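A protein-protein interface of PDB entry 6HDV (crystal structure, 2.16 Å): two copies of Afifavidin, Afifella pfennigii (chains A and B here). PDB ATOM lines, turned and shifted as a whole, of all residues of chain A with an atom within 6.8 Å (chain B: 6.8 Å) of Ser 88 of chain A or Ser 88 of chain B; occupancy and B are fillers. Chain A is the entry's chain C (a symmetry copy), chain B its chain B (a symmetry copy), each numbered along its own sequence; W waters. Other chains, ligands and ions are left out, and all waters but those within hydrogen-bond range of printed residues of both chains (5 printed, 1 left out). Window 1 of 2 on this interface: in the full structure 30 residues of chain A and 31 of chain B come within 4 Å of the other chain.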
ATOM      1  N   LEU A  64     -33.072  28.896   6.538  1.00  0.00           N
ATOM      2  CA  LEU A  64     -34.390  29.095   6.017  1.00  0.00           C
ATOM      3  C   LEU A  64     -35.411  29.053   7.152  1.00  0.00           C
ATOM      4  O   LEU A  64     -35.188  28.451   8.197  1.00  0.00           O
ATOM      5  CB  LEU A  64     -34.732  27.981   5.017  1.00  0.00           C
ATOM      6  CG  LEU A  64     -33.796  27.844   3.822  1.00  0.00           C
ATOM      7  CD1 LEU A  64     -34.084  26.553   3.060  1.00  0.00           C
ATOM      8  CD2 LEU A  64     -33.872  29.072   2.895  1.00  0.00           C
ATOM      9  N   ILE A  70     -37.584  27.668  12.035  1.00  0.00           N
ATOM     10  CA  ILE A  70     -36.354  28.130  11.504  1.00  0.00           C
ATOM     11  C   ILE A  70     -35.315  27.040  11.681  1.00  0.00           C
ATOM     12  O   ILE A  70     -35.358  26.341  12.636  1.00  0.00           O
ATOM     13  CB  ILE A  70     -35.882  29.439  12.204  1.00  0.00           C
ATOM     14  CG1 ILE A  70     -34.706  30.107  11.483  1.00  0.00           C
ATOM     15  CG2 ILE A  70     -35.535  29.214  13.663  1.00  0.00           C
ATOM     16  CD1 ILE A  70     -34.435  31.569  11.922  1.00  0.00           C
ATOM     17  N   GLY A  71     -34.370  27.005  10.749  1.00  0.00           N
ATOM     18  CA  GLY A  71     -33.099  26.386  10.923  1.00  0.00           C
ATOM     19  C   GLY A  71     -32.018  27.202  10.212  1.00  0.00           C
ATOM     20  O   GLY A  71     -32.281  27.917   9.242  1.00  0.00           O
ATOM     21  N   PHE A  72     -30.798  27.115  10.731  1.00  0.00           N
ATOM     22  CA  PHE A  72     -29.686  27.876  10.229  1.00  0.00           C
ATOM     23  C   PHE A  72     -28.407  27.148  10.648  1.00  0.00           C
ATOM     24  O   PHE A  72     -28.444  26.391  11.626  1.00  0.00           O
ATOM     25  CB  PHE A  72     -29.756  29.326  10.740  1.00  0.00           C
ATOM     26  CG  PHE A  72     -29.788  29.508  12.243  1.00  0.00           C
ATOM     27  CD1 PHE A  72     -28.623  29.574  12.995  1.00  0.00           C
ATOM     28  CD2 PHE A  72     -30.983  29.627  12.920  1.00  0.00           C
ATOM     29  CE1 PHE A  72     -28.639  29.773  14.378  1.00  0.00           C
ATOM     30  CE2 PHE A  72     -31.011  29.832  14.294  1.00  0.00           C
ATOM     31  CZ  PHE A  72     -29.838  29.925  15.024  1.00  0.00           C
ATOM     32  N   THR A  73     -27.322  27.329   9.890  1.00  0.00           N
ATOM     33  CA  THR A  73     -26.050  26.746  10.219  1.00  0.00           C
ATOM     34  C   THR A  73     -24.933  27.796  10.242  1.00  0.00           C
ATOM     35  O   THR A  73     -25.039  28.929   9.710  1.00  0.00           O
ATOM     36  CB  THR A  73     -25.773  25.495   9.388  1.00  0.00           C
ATOM     37  OG1 THR A  73     -24.559  25.665   8.682  1.00  0.00           O
ATOM     38  CG2 THR A  73     -26.931  25.122   8.496  1.00  0.00           C
ATOM     39  N   VAL A  74     -23.907  27.457  11.029  1.00  0.00           N
ATOM     40  CA  VAL A  74     -22.732  28.258  11.189  1.00  0.00           C
ATOM     41  C   VAL A  74     -21.540  27.338  10.944  1.00  0.00           C
ATOM     42  O   VAL A  74     -21.468  26.292  11.558  1.00  0.00           O
ATOM     43  CB  VAL A  74     -22.649  28.895  12.594  1.00  0.00           C
ATOM     44  CG1 VAL A  74     -21.255  29.444  12.889  1.00  0.00           C
ATOM     45  CG2 VAL A  74     -23.689  29.992  12.821  1.00  0.00           C
ATOM     46  N   TRP A  76     -17.590  27.175  11.656  1.00  0.00           N
ATOM     47  CA  TRP A  76     -16.667  27.809  12.546  1.00  0.00           C
ATOM     48  C   TRP A  76     -15.402  28.114  11.766  1.00  0.00           C
ATOM     49  O   TRP A  76     -14.344  27.527  12.013  1.00  0.00           O
ATOM     50  CB  TRP A  76     -16.447  26.942  13.782  1.00  0.00           C
ATOM     51  CG  TRP A  76     -17.764  26.722  14.445  1.00  0.00           C
ATOM     52  CD1 TRP A  76     -18.500  25.569  14.477  1.00  0.00           C
ATOM     53  CD2 TRP A  76     -18.577  27.746  15.037  1.00  0.00           C
ATOM     54  NE1 TRP A  76     -19.696  25.813  15.094  1.00  0.00           N
ATOM     55  CE2 TRP A  76     -19.774  27.133  15.441  1.00  0.00           C
ATOM     56  CE3 TRP A  76     -18.414  29.116  15.233  1.00  0.00           C
ATOM     57  CZ2 TRP A  76     -20.808  27.833  16.051  1.00  0.00           C
ATOM     58  CZ3 TRP A  76     -19.429  29.807  15.848  1.00  0.00           C
ATOM     59  CH2 TRP A  76     -20.604  29.169  16.262  1.00  0.00           C
ATOM     60  N   VAL A  86     -19.000  22.465  12.150  1.00  0.00           N
ATOM     61  CA  VAL A  86     -20.123  23.297  11.832  1.00  0.00           C
ATOM     62  C   VAL A  86     -21.283  22.872  12.725  1.00  0.00           C
ATOM     63  O   VAL A  86     -21.348  21.710  13.114  1.00  0.00           O
ATOM     64  CB  VAL A  86     -20.497  23.306  10.329  1.00  0.00           C
ATOM     65  CG1 VAL A  86     -19.558  22.517   9.453  1.00  0.00           C
ATOM     66  CG2 VAL A  86     -21.938  22.937  10.080  1.00  0.00           C
ATOM     67  N   THR A  87     -22.170  23.827  13.016  1.00  0.00           N
ATOM     68  CA  THR A  87     -23.303  23.638  13.864  1.00  0.00           C
ATOM     69  C   THR A  87     -24.556  24.036  13.106  1.00  0.00           C
ATOM     70  O   THR A  87     -24.523  25.030  12.449  1.00  0.00           O
ATOM     71  CB  THR A  87     -23.199  24.515  15.119  1.00  0.00           C
ATOM     72  OG1 THR A  87     -22.121  24.010  15.886  1.00  0.00           O
ATOM     73  CG2 THR A  87     -24.453  24.547  15.966  1.00  0.00           C
ATOM     74  N   SER A  88     -25.653  23.275  13.241  1.00  0.00           N
ATOM     75  CA  SER A  88     -26.953  23.767  12.785  1.00  0.00           C
ATOM     76  C   SER A  88     -27.955  23.772  13.938  1.00  0.00           C
ATOM     77  O   SER A  88     -28.013  22.831  14.764  1.00  0.00           O
ATOM     78  CB  SER A  88     -27.497  22.988  11.613  1.00  0.00           C
ATOM     79  OG  SER A  88     -26.513  22.787  10.626  1.00  0.00           O
ATOM     80  N   TRP A  89     -28.770  24.825  13.959  1.00  0.00           N
ATOM     81  CA  TRP A  89     -29.806  24.980  14.921  1.00  0.00           C
ATOM     82  C   TRP A  89     -31.114  24.779  14.187  1.00  0.00           C
ATOM     83  O   TRP A  89     -31.259  25.221  13.023  1.00  0.00           O
ATOM     84  CB  TRP A  89     -29.829  26.377  15.525  1.00  0.00           C
ATOM     85  CG  TRP A  89     -28.748  26.732  16.485  1.00  0.00           C
ATOM     86  CD1 TRP A  89     -28.871  26.888  17.837  1.00  0.00           C
ATOM     87  CD2 TRP A  89     -27.409  27.111  16.149  1.00  0.00           C
ATOM     88  NE1 TRP A  89     -27.671  27.247  18.382  1.00  0.00           N
ATOM     89  CE2 TRP A  89     -26.760  27.421  17.366  1.00  0.00           C
ATOM     90  CE3 TRP A  89     -26.708  27.259  14.948  1.00  0.00           C
ATOM     91  CZ2 TRP A  89     -25.435  27.862  17.402  1.00  0.00           C
ATOM     92  CZ3 TRP A  89     -25.395  27.673  14.990  1.00  0.00           C
ATOM     93  CH2 TRP A  89     -24.767  27.959  16.205  1.00  0.00           C
ATOM     94  N   THR A  90     -32.082  24.166  14.875  1.00  0.00           N
ATOM     95  CA  THR A  90     -33.402  24.121  14.361  1.00  0.00           C
ATOM     96  C   THR A  90     -34.366  24.371  15.485  1.00  0.00           C
ATOM     97  O   THR A  90     -34.093  23.904  16.555  1.00  0.00           O
ATOM     98  CB  THR A  90     -33.679  22.750  13.776  1.00  0.00           C
ATOM     99  OG1 THR A  90     -32.503  22.360  13.082  1.00  0.00           O
ATOM    100  CG2 THR A  90     -34.920  22.731  12.915  1.00  0.00           C
ATOM    101  N   GLY A  91     -35.490  25.032  15.213  1.00  0.00           N
ATOM    102  CA  GLY A  91     -36.418  25.299  16.290  1.00  0.00           C
ATOM    103  C   GLY A  91     -37.574  26.190  15.883  1.00  0.00           C
ATOM    104  O   GLY A  91     -37.843  26.360  14.716  1.00  0.00           O
ATOM    105  N   ASP A 105     -32.756  23.263  19.150  1.00  0.00           N
ATOM    106  CA  ASP A 105     -31.783  22.266  19.446  1.00  0.00           C
ATOM    107  C   ASP A 105     -30.701  22.412  18.390  1.00  0.00           C
ATOM    108  O   ASP A 105     -30.985  22.894  17.276  1.00  0.00           O
ATOM    109  CB  ASP A 105     -32.362  20.829  19.405  1.00  0.00           C
ATOM    110  CG  ASP A 105     -33.217  20.419  20.612  1.00  0.00           C
ATOM    111  OD1 ASP A 105     -33.154  21.136  21.688  1.00  0.00           O
ATOM    112  OD2 ASP A 105     -33.983  19.398  20.459  1.00  0.00           O
ATOM    113  N   TRP A 106     -29.522  21.887  18.693  1.00  0.00           N
ATOM    114  CA  TRP A 106     -28.437  22.014  17.764  1.00  0.00           C
ATOM    115  C   TRP A 106     -27.538  20.760  17.746  1.00  0.00           C
ATOM    116  O   TRP A 106     -27.393  20.001  18.706  1.00  0.00           O
ATOM    117  CB  TRP A 106     -27.624  23.301  18.052  1.00  0.00           C
ATOM    118  CG  TRP A 106     -27.076  23.445  19.451  1.00  0.00           C
ATOM    119  CD1 TRP A 106     -27.569  24.228  20.457  1.00  0.00           C
ATOM    120  CD2 TRP A 106     -25.898  22.825  20.005  1.00  0.00           C
ATOM    121  NE1 TRP A 106     -26.775  24.145  21.577  1.00  0.00           N
ATOM    122  CE2 TRP A 106     -25.741  23.298  21.314  1.00  0.00           C
ATOM    123  CE3 TRP A 106     -24.954  21.922  19.501  1.00  0.00           C
ATOM    124  CZ2 TRP A 106     -24.716  22.877  22.144  1.00  0.00           C
ATOM    125  CZ3 TRP A 106     -23.923  21.510  20.309  1.00  0.00           C
ATOM    126  CH2 TRP A 106     -23.796  22.001  21.612  1.00  0.00           C
ATOM    127  N   ASN A 107     -26.867  20.584  16.612  1.00  0.00           N
ATOM    128  CA  ASN A 107     -25.951  19.565  16.421  1.00  0.00           C
ATOM    129  C   ASN A 107     -24.682  20.258  15.972  1.00  0.00           C
ATOM    130  O   ASN A 107     -24.747  21.163  15.131  1.00  0.00           O
ATOM    131  CB  ASN A 107     -26.476  18.573  15.385  1.00  0.00           C
ATOM    132  CG  ASN A 107     -27.525  17.632  15.947  1.00  0.00           C
ATOM    133  OD1 ASN A 107     -27.359  17.075  17.050  1.00  0.00           O
ATOM    134  ND2 ASN A 107     -28.608  17.452  15.200  1.00  0.00           N
ATOM    135  N   LEU A 108     -23.566  19.793  16.522  1.00  0.00           N
ATOM    136  CA  LEU A 108     -22.258  20.266  16.210  1.00  0.00           C
ATOM    137  C   LEU A 108     -21.457  19.074  15.713  1.00  0.00           C
ATOM    138  O   LEU A 108     -21.245  18.168  16.469  1.00  0.00           O
ATOM    139  CB  LEU A 108     -21.604  20.835  17.467  1.00  0.00           C
ATOM    140  CG  LEU A 108     -20.097  21.108  17.363  1.00  0.00           C
ATOM    141  CD1 LEU A 108     -19.805  22.253  16.394  1.00  0.00           C
ATOM    142  CD2 LEU A 108     -19.505  21.459  18.727  1.00  0.00           C
ATOM    143  N   ALA A 109     -21.084  19.109  14.432  1.00  0.00           N
ATOM    144  CA  ALA A 109     -20.278  18.094  13.797  1.00  0.00           C
ATOM    145  C   ALA A 109     -18.820  18.564  13.799  1.00  0.00           C
ATOM    146  O   ALA A 109     -18.556  19.728  13.449  1.00  0.00           O
ATOM    147  CB  ALA A 109     -20.787  17.811  12.405  1.00  0.00           C
ATOM    148  N   LEU B  64     -23.754  25.551   5.006  1.00  0.00           N
ATOM    149  CA  LEU B  64     -22.375  25.876   4.947  1.00  0.00           C
ATOM    150  C   LEU B  64     -21.554  24.618   5.181  1.00  0.00           C
ATOM    151  O   LEU B  64     -22.037  23.679   5.767  1.00  0.00           O
ATOM    152  CB  LEU B  64     -22.040  26.924   6.017  1.00  0.00           C
ATOM    153  CG  LEU B  64     -22.762  28.262   5.876  1.00  0.00           C
ATOM    154  CD1 LEU B  64     -22.489  29.146   7.083  1.00  0.00           C
ATOM    155  CD2 LEU B  64     -22.339  28.967   4.589  1.00  0.00           C
ATOM    156  N   ILE B  70     -20.450  19.687   7.422  1.00  0.00           N
ATOM    157  CA  ILE B  70     -21.530  20.304   6.689  1.00  0.00           C
ATOM    158  C   ILE B  70     -22.749  20.479   7.585  1.00  0.00           C
ATOM    159  O   ILE B  70     -23.063  19.647   8.402  1.00  0.00           O
ATOM    160  CB  ILE B  70     -21.879  19.472   5.435  1.00  0.00           C
ATOM    161  CG1 ILE B  70     -22.797  20.230   4.483  1.00  0.00           C
ATOM    162  CG2 ILE B  70     -22.500  18.133   5.779  1.00  0.00           C
ATOM    163  CD1 ILE B  70     -22.600  19.831   3.035  1.00  0.00           C
ATOM    164  N   GLY B  71     -23.503  21.526   7.296  1.00  0.00           N
ATOM    165  CA  GLY B  71     -24.849  21.717   7.805  1.00  0.00           C
ATOM    166  C   GLY B  71     -25.761  22.343   6.760  1.00  0.00           C
ATOM    167  O   GLY B  71     -25.322  23.208   5.955  1.00  0.00           O
ATOM    168  N   PHE B  72     -27.019  21.885   6.717  1.00  0.00           N
ATOM    169  CA  PHE B  72     -27.943  22.476   5.810  1.00  0.00           C
ATOM    170  C   PHE B  72     -29.366  22.347   6.325  1.00  0.00           C
ATOM    171  O   PHE B  72     -29.631  21.466   7.091  1.00  0.00           O
ATOM    172  CB  PHE B  72     -27.802  21.868   4.417  1.00  0.00           C
ATOM    173  CG  PHE B  72     -27.967  20.378   4.338  1.00  0.00           C
ATOM    174  CD1 PHE B  72     -29.212  19.814   4.107  1.00  0.00           C
ATOM    175  CD2 PHE B  72     -26.868  19.541   4.416  1.00  0.00           C
ATOM    176  CE1 PHE B  72     -29.352  18.444   3.979  1.00  0.00           C
ATOM    177  CE2 PHE B  72     -27.014  18.167   4.326  1.00  0.00           C
ATOM    178  CZ  PHE B  72     -28.251  17.624   4.113  1.00  0.00           C
ATOM    179  N   THR B  73     -30.230  23.220   5.790  1.00  0.00           N
ATOM    180  CA  THR B  73     -31.613  23.395   6.128  1.00  0.00           C
ATOM    181  C   THR B  73     -32.477  23.330   4.857  1.00  0.00           C
ATOM    182  O   THR B  73     -32.091  23.871   3.835  1.00  0.00           O
ATOM    183  CB  THR B  73     -31.786  24.730   6.863  1.00  0.00           C
ATOM    184  OG1 THR B  73     -30.953  24.669   8.012  1.00  0.00           O
ATOM    185  CG2 THR B  73     -33.194  25.072   7.302  1.00  0.00           C
ATOM    186  N   VAL B  74     -33.621  22.626   4.968  1.00  0.00           N
ATOM    187  CA  VAL B  74     -34.792  22.673   4.114  1.00  0.00           C
ATOM    188  C   VAL B  74     -36.005  23.157   4.911  1.00  0.00           C
ATOM    189  O   VAL B  74     -36.352  22.579   5.930  1.00  0.00           O
ATOM    190  CB  VAL B  74     -35.139  21.280   3.559  1.00  0.00           C
ATOM    191  CG1 VAL B  74     -36.389  21.312   2.703  1.00  0.00           C
ATOM    192  CG2 VAL B  74     -33.989  20.653   2.810  1.00  0.00           C
ATOM    193  N   TRP B  76     -40.016  23.105   4.476  1.00  0.00           N
ATOM    194  CA  TRP B  76     -41.000  22.247   3.787  1.00  0.00           C
ATOM    195  C   TRP B  76     -42.078  23.149   3.168  1.00  0.00           C
ATOM    196  O   TRP B  76     -43.256  23.120   3.528  1.00  0.00           O
ATOM    197  CB  TRP B  76     -41.552  21.138   4.726  1.00  0.00           C
ATOM    198  CG  TRP B  76     -40.417  20.293   5.208  1.00  0.00           C
ATOM    199  CD1 TRP B  76     -39.868  20.297   6.455  1.00  0.00           C
ATOM    200  CD2 TRP B  76     -39.533  19.500   4.389  1.00  0.00           C
ATOM    201  NE1 TRP B  76     -38.724  19.538   6.474  1.00  0.00           N
ATOM    202  CE2 TRP B  76     -38.506  19.018   5.227  1.00  0.00           C
ATOM    203  CE3 TRP B  76     -39.531  19.111   3.039  1.00  0.00           C
ATOM    204  CZ2 TRP B  76     -37.493  18.182   4.769  1.00  0.00           C
ATOM    205  CZ3 TRP B  76     -38.546  18.249   2.593  1.00  0.00           C
ATOM    206  CH2 TRP B  76     -37.537  17.797   3.452  1.00  0.00           C
ATOM    207  N   VAL B  86     -39.497  22.880   9.283  1.00  0.00           N
ATOM    208  CA  VAL B  86     -38.159  22.977   8.678  1.00  0.00           C
ATOM    209  C   VAL B  86     -37.270  21.941   9.329  1.00  0.00           C
ATOM    210  O   VAL B  86     -37.452  21.615  10.483  1.00  0.00           O
ATOM    211  CB  VAL B  86     -37.520  24.386   8.696  1.00  0.00           C
ATOM    212  CG1 VAL B  86     -38.425  25.488   9.180  1.00  0.00           C
ATOM    213  CG2 VAL B  86     -36.201  24.441   9.403  1.00  0.00           C
ATOM    214  N   THR B  87     -36.299  21.459   8.553  1.00  0.00           N
ATOM    215  CA  THR B  87     -35.393  20.456   9.014  1.00  0.00           C
ATOM    216  C   THR B  87     -33.973  20.930   8.785  1.00  0.00           C
ATOM    217  O   THR B  87     -33.704  21.600   7.749  1.00  0.00           O
ATOM    218  CB  THR B  87     -35.609  19.129   8.289  1.00  0.00           C
ATOM    219  OG1 THR B  87     -36.919  18.721   8.669  1.00  0.00           O
ATOM    220  CG2 THR B  87     -34.569  18.076   8.609  1.00  0.00           C
ATOM    221  N   SER B  88     -33.093  20.614   9.758  1.00  0.00           N
ATOM    222  CA  SER B  88     -31.675  20.895   9.595  1.00  0.00           C
ATOM    223  C   SER B  88     -30.902  19.614   9.826  1.00  0.00           C
ATOM    224  O   SER B  88     -31.237  18.848  10.715  1.00  0.00           O
ATOM    225  CB  SER B  88     -31.144  22.031  10.464  1.00  0.00           C
ATOM    226  OG  SER B  88     -31.822  23.269  10.256  1.00  0.00           O
ATOM    227  N   TRP B  89     -29.892  19.423   8.984  1.00  0.00           N
ATOM    228  CA  TRP B  89     -28.999  18.283   8.986  1.00  0.00           C
ATOM    229  C   TRP B  89     -27.611  18.760   9.351  1.00  0.00           C
ATOM    230  O   TRP B  89     -27.145  19.771   8.846  1.00  0.00           O
ATOM    231  CB  TRP B  89     -28.932  17.661   7.586  1.00  0.00           C
ATOM    232  CG  TRP B  89     -30.092  16.840   7.134  1.00  0.00           C
ATOM    233  CD1 TRP B  89     -30.185  15.475   7.179  1.00  0.00           C
ATOM    234  CD2 TRP B  89     -31.310  17.302   6.543  1.00  0.00           C
ATOM    235  NE1 TRP B  89     -31.399  15.061   6.712  1.00  0.00           N
ATOM    236  CE2 TRP B  89     -32.098  16.150   6.267  1.00  0.00           C
ATOM    237  CE3 TRP B  89     -31.814  18.560   6.199  1.00  0.00           C
ATOM    238  CZ2 TRP B  89     -33.347  16.218   5.644  1.00  0.00           C
ATOM    239  CZ3 TRP B  89     -33.058  18.628   5.589  1.00  0.00           C
ATOM    240  CH2 TRP B  89     -33.817  17.480   5.324  1.00  0.00           C
ATOM    241  N   THR B  90     -26.911  17.996  10.157  1.00  0.00           N
ATOM    242  CA  THR B  90     -25.552  18.323  10.390  1.00  0.00           C
ATOM    243  C   THR B  90     -24.724  17.039  10.464  1.00  0.00           C
ATOM    244  O   THR B  90     -25.130  16.044  11.066  1.00  0.00           O
ATOM    245  CB  THR B  90     -25.407  19.124  11.681  1.00  0.00           C
ATOM    246  OG1 THR B  90     -26.400  20.148  11.795  1.00  0.00           O
ATOM    247  CG2 THR B  90     -24.004  19.671  11.744  1.00  0.00           C
ATOM    248  N   GLY B  91     -23.530  17.063   9.896  1.00  0.00           N
ATOM    249  CA  GLY B  91     -22.800  15.831   9.831  1.00  0.00           C
ATOM    250  C   GLY B  91     -21.452  15.967   9.169  1.00  0.00           C
ATOM    251  O   GLY B  91     -20.937  17.098   9.000  1.00  0.00           O
ATOM    252  N   ASP B 105     -27.055  13.728  11.678  1.00  0.00           N
ATOM    253  CA  ASP B 105     -28.160  13.820  12.561  1.00  0.00           C
ATOM    254  C   ASP B 105     -28.996  15.038  12.179  1.00  0.00           C
ATOM    255  O   ASP B 105     -28.462  16.046  11.704  1.00  0.00           O
ATOM    256  CB  ASP B 105     -27.681  13.981  14.012  1.00  0.00           C
ATOM    257  CG  ASP B 105     -26.861  12.804  14.512  1.00  0.00           C
ATOM    258  OD1 ASP B 105     -27.133  11.659  14.037  1.00  0.00           O
ATOM    259  OD2 ASP B 105     -25.984  13.038  15.376  1.00  0.00           O
ATOM    260  N   TRP B 106     -30.300  14.987  12.447  1.00  0.00           N
ATOM    261  CA  TRP B 106     -31.217  16.023  11.987  1.00  0.00           C
ATOM    262  C   TRP B 106     -32.284  16.312  13.034  1.00  0.00           C
ATOM    263  O   TRP B 106     -32.614  15.483  13.890  1.00  0.00           O
ATOM    264  CB  TRP B 106     -31.887  15.640  10.643  1.00  0.00           C
ATOM    265  CG  TRP B 106     -32.576  14.292  10.594  1.00  0.00           C
ATOM    266  CD1 TRP B 106     -32.081  13.135  10.050  1.00  0.00           C
ATOM    267  CD2 TRP B 106     -33.896  13.959  11.047  1.00  0.00           C
ATOM    268  NE1 TRP B 106     -32.986  12.123  10.133  1.00  0.00           N
ATOM    269  CE2 TRP B 106     -34.120  12.606  10.727  1.00  0.00           C
ATOM    270  CE3 TRP B 106     -34.907  14.677  11.681  1.00  0.00           C
ATOM    271  CZ2 TRP B 106     -35.292  11.937  11.080  1.00  0.00           C
ATOM    272  CZ3 TRP B 106     -36.060  14.019  12.046  1.00  0.00           C
ATOM    273  CH2 TRP B 106     -36.256  12.669  11.734  1.00  0.00           C
ATOM    274  N   ASN B 107     -32.886  17.476  12.858  1.00  0.00           N
ATOM    275  CA  ASN B 107     -33.870  17.982  13.696  1.00  0.00           C
ATOM    276  C   ASN B 107     -34.936  18.579  12.811  1.00  0.00           C
ATOM    277  O   ASN B 107     -34.604  19.283  11.860  1.00  0.00           O
ATOM    278  CB  ASN B 107     -33.317  19.041  14.653  1.00  0.00           C
ATOM    279  CG  ASN B 107     -32.491  18.458  15.778  1.00  0.00           C
ATOM    280  OD1 ASN B 107     -32.858  17.447  16.428  1.00  0.00           O
ATOM    281  ND2 ASN B 107     -31.358  19.093  16.003  1.00  0.00           N
ATOM    282  N   LEU B 108     -36.184  18.300  13.169  1.00  0.00           N
ATOM    283  CA  LEU B 108     -37.337  18.777  12.461  1.00  0.00           C
ATOM    284  C   LEU B 108     -38.222  19.503  13.452  1.00  0.00           C
ATOM    285  O   LEU B 108     -38.695  18.902  14.420  1.00  0.00           O
ATOM    286  CB  LEU B 108     -38.104  17.589  11.872  1.00  0.00           C
ATOM    287  CG  LEU B 108     -39.529  17.873  11.369  1.00  0.00           C
ATOM    288  CD1 LEU B 108     -39.527  18.658  10.067  1.00  0.00           C
ATOM    289  CD2 LEU B 108     -40.296  16.583  11.158  1.00  0.00           C
ATOM    290  N   ALA B 109     -38.441  20.777  13.199  1.00  0.00           N
ATOM    291  CA  ALA B 109     -39.234  21.593  14.067  1.00  0.00           C
ATOM    292  C   ALA B 109     -40.554  21.745  13.370  1.00  0.00           C
ATOM    293  O   ALA B 109     -40.533  21.988  12.198  1.00  0.00           O
ATOM    294  CB  ALA B 109     -38.590  22.930  14.289  1.00  0.00           C
HETATM  295  O   HOH W   1     -30.375  15.308  15.707  1.00  0.00           O
HETATM  296  O   HOH W   2     -29.919  17.850  18.047  1.00  0.00           O
HETATM  297  O   HOH W   3     -33.090  17.095  19.163  1.00  0.00           O
HETATM  298  O   HOH W   4     -29.052  19.586  12.681  1.00  0.00           O
HETATM  299  O   HOH W   5     -30.331  21.463  14.163  1.00  0.00           O
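CG2 of Thr 73 of chain A touches N of Phe 72 of chain B, 3.7 Å away.
OG of Ser 88 of chain A touches CA of Gly 71 of chain B, at 3.4 Å.
Ser 88 of chain A touches Ser 88 of chain B.
Asn 107 of chain B touches Thr 90 of chain A.
Thr 90 of chain A touches Ala 109 of chain B.
Asp 105 of chain A touches Asn 107 of chain B.
Asn 107 of chain A touches Thr 90 of chain B.
O of Asp 105 of chain B touches ND2 of Asn 107 of chain A (3.8 Å).
Ala 109 of chain A touches Thr 90 of chain B.
Ala 109 of chain A touches Gly 91 of chain B.
Printed residues of chain A that touch a printed residue of chain B: Leu 64, Ile 70, Gly 71, Phe 72, Thr 73, Val 86, Ser 88, Trp 89, Thr 90, Gly 91, Asp 105, Asn 107 and Ala 109.
Among the printed residues, 28 pairs touch across the chains.
Among the printed residues, no Asp or Glu carboxylate lies within 4 Å of a Lys or Arg side-chain nitrogen of the other chain.
OG of Ser 88 of chain B sits close to OG1 of Thr 90 of chain A, 3.0 Å away.
The side-chain amide nitrogen (ND2) of Asn 107 of chain B lies close to the side-chain amide nitrogen (ND2) of Asn 107 of chain A (3.3 Å).
The side-chain hydroxyl of Ser 88 of chain A sits at hydrogen-bond distance from the side-chain hydroxyl of Thr 90 of chain B (2.9 Å).
O of Trp 89 of chain A is in hydrogen-bond range of OG of Ser 88 of chain B (3.4 Å).
Ser 88 of chain A touches just these residues of chain B: Gly 71 (3.4 Å), Ser 88 (3.9 Å), Trp 89 (3.6 Å) and Thr 90 (2.9 Å).
Of the printed residues of chain B, Trp 89 of chain A touches Ser 88.
Printed residues of chain A within 4 Å of Leu 64 of chain B: Thr 73 (3.7 Å).
Trp 76 of chain B touches none of the printed residues of chain A.
Printed residues of chain A within 4 Å of Ser 88 of chain B: Gly 71 (3.4 Å), Ser 88 (3.9 Å), Trp 89 (3.4 Å) and Thr 90 (3.0 Å).
Trp 106 of chain B touches none of the printed residues of chain A.
The nearest residue of chain B that does not touch Ser 88 of chain A is Phe 72 of chain B (4.04 Å).
The nearest printed residue of chain A that does not touch Ser 88 of chain B is Phe 72 of chain A (4.01 Å).
Water W2 lies within hydrogen-bond range of ND2 of Asn 107 of chain B (2.8 Å), OD1 of Asn 107 of chain A (2.9 Å) and O of Trp 106 of chain A (3.4 Å).
Water W1 lies within hydrogen-bond range of the side-chain amide nitrogen of Asn 107 of chain A (2.8 Å), the backbone carbonyl oxygen of Trp 106 of chain B (2.9 Å) and the side-chain amide oxygen of Asn 107 of chain B (3.4 Å).
Water W4 lies within hydrogen-bond range of OG1 of Thr 90 of chain B (2.9 Å), O of Ser 88 of chain B (3.0 Å) and ND2 of Asn 107 of chain A (3.3 Å).
Leu 64 of chain A touches Thr 73 of chain B, and with the chains exchanged Thr 73 of chain A touches Leu 64 of chain B.
Ile 70 of chain A touches Val 86 of chain B, and with the chains exchanged Val 86 of chain A touches Ile 70 of chain B.
Thr 90 of chain A touches Ala 109 of chain B, and with the chains exchanged Ala 109 of chain A touches Thr 90 of chain B.
Of the 28 pairs that touch across the chains among the printed residues, 28 have their exchanged pair printed and touching as well.
The backbone carbonyl oxygen of Ile 70 of chain B lies within hydrogen-bond range of the backbone NH of Gly 91 of chain B (3.0 Å).
The backbone NH (N) of Ser 88 of chain A lies within hydrogen-bond range of the backbone carbonyl oxygen (O) of Asn 107 of chain A (3.0 Å).
N of Ala 109 of chain B is in hydrogen-bond range of O of Val 86 of chain B, 3.0 Å away.
O of Val 86 of chain A lies within hydrogen-bond range of N of Ala 109 of chain A (2.9 Å).
The backbone carbonyl oxygen of Phe 72 of chain A is in hydrogen-bond range of the backbone NH of Trp 89 of chain A, at 2.8 Å.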
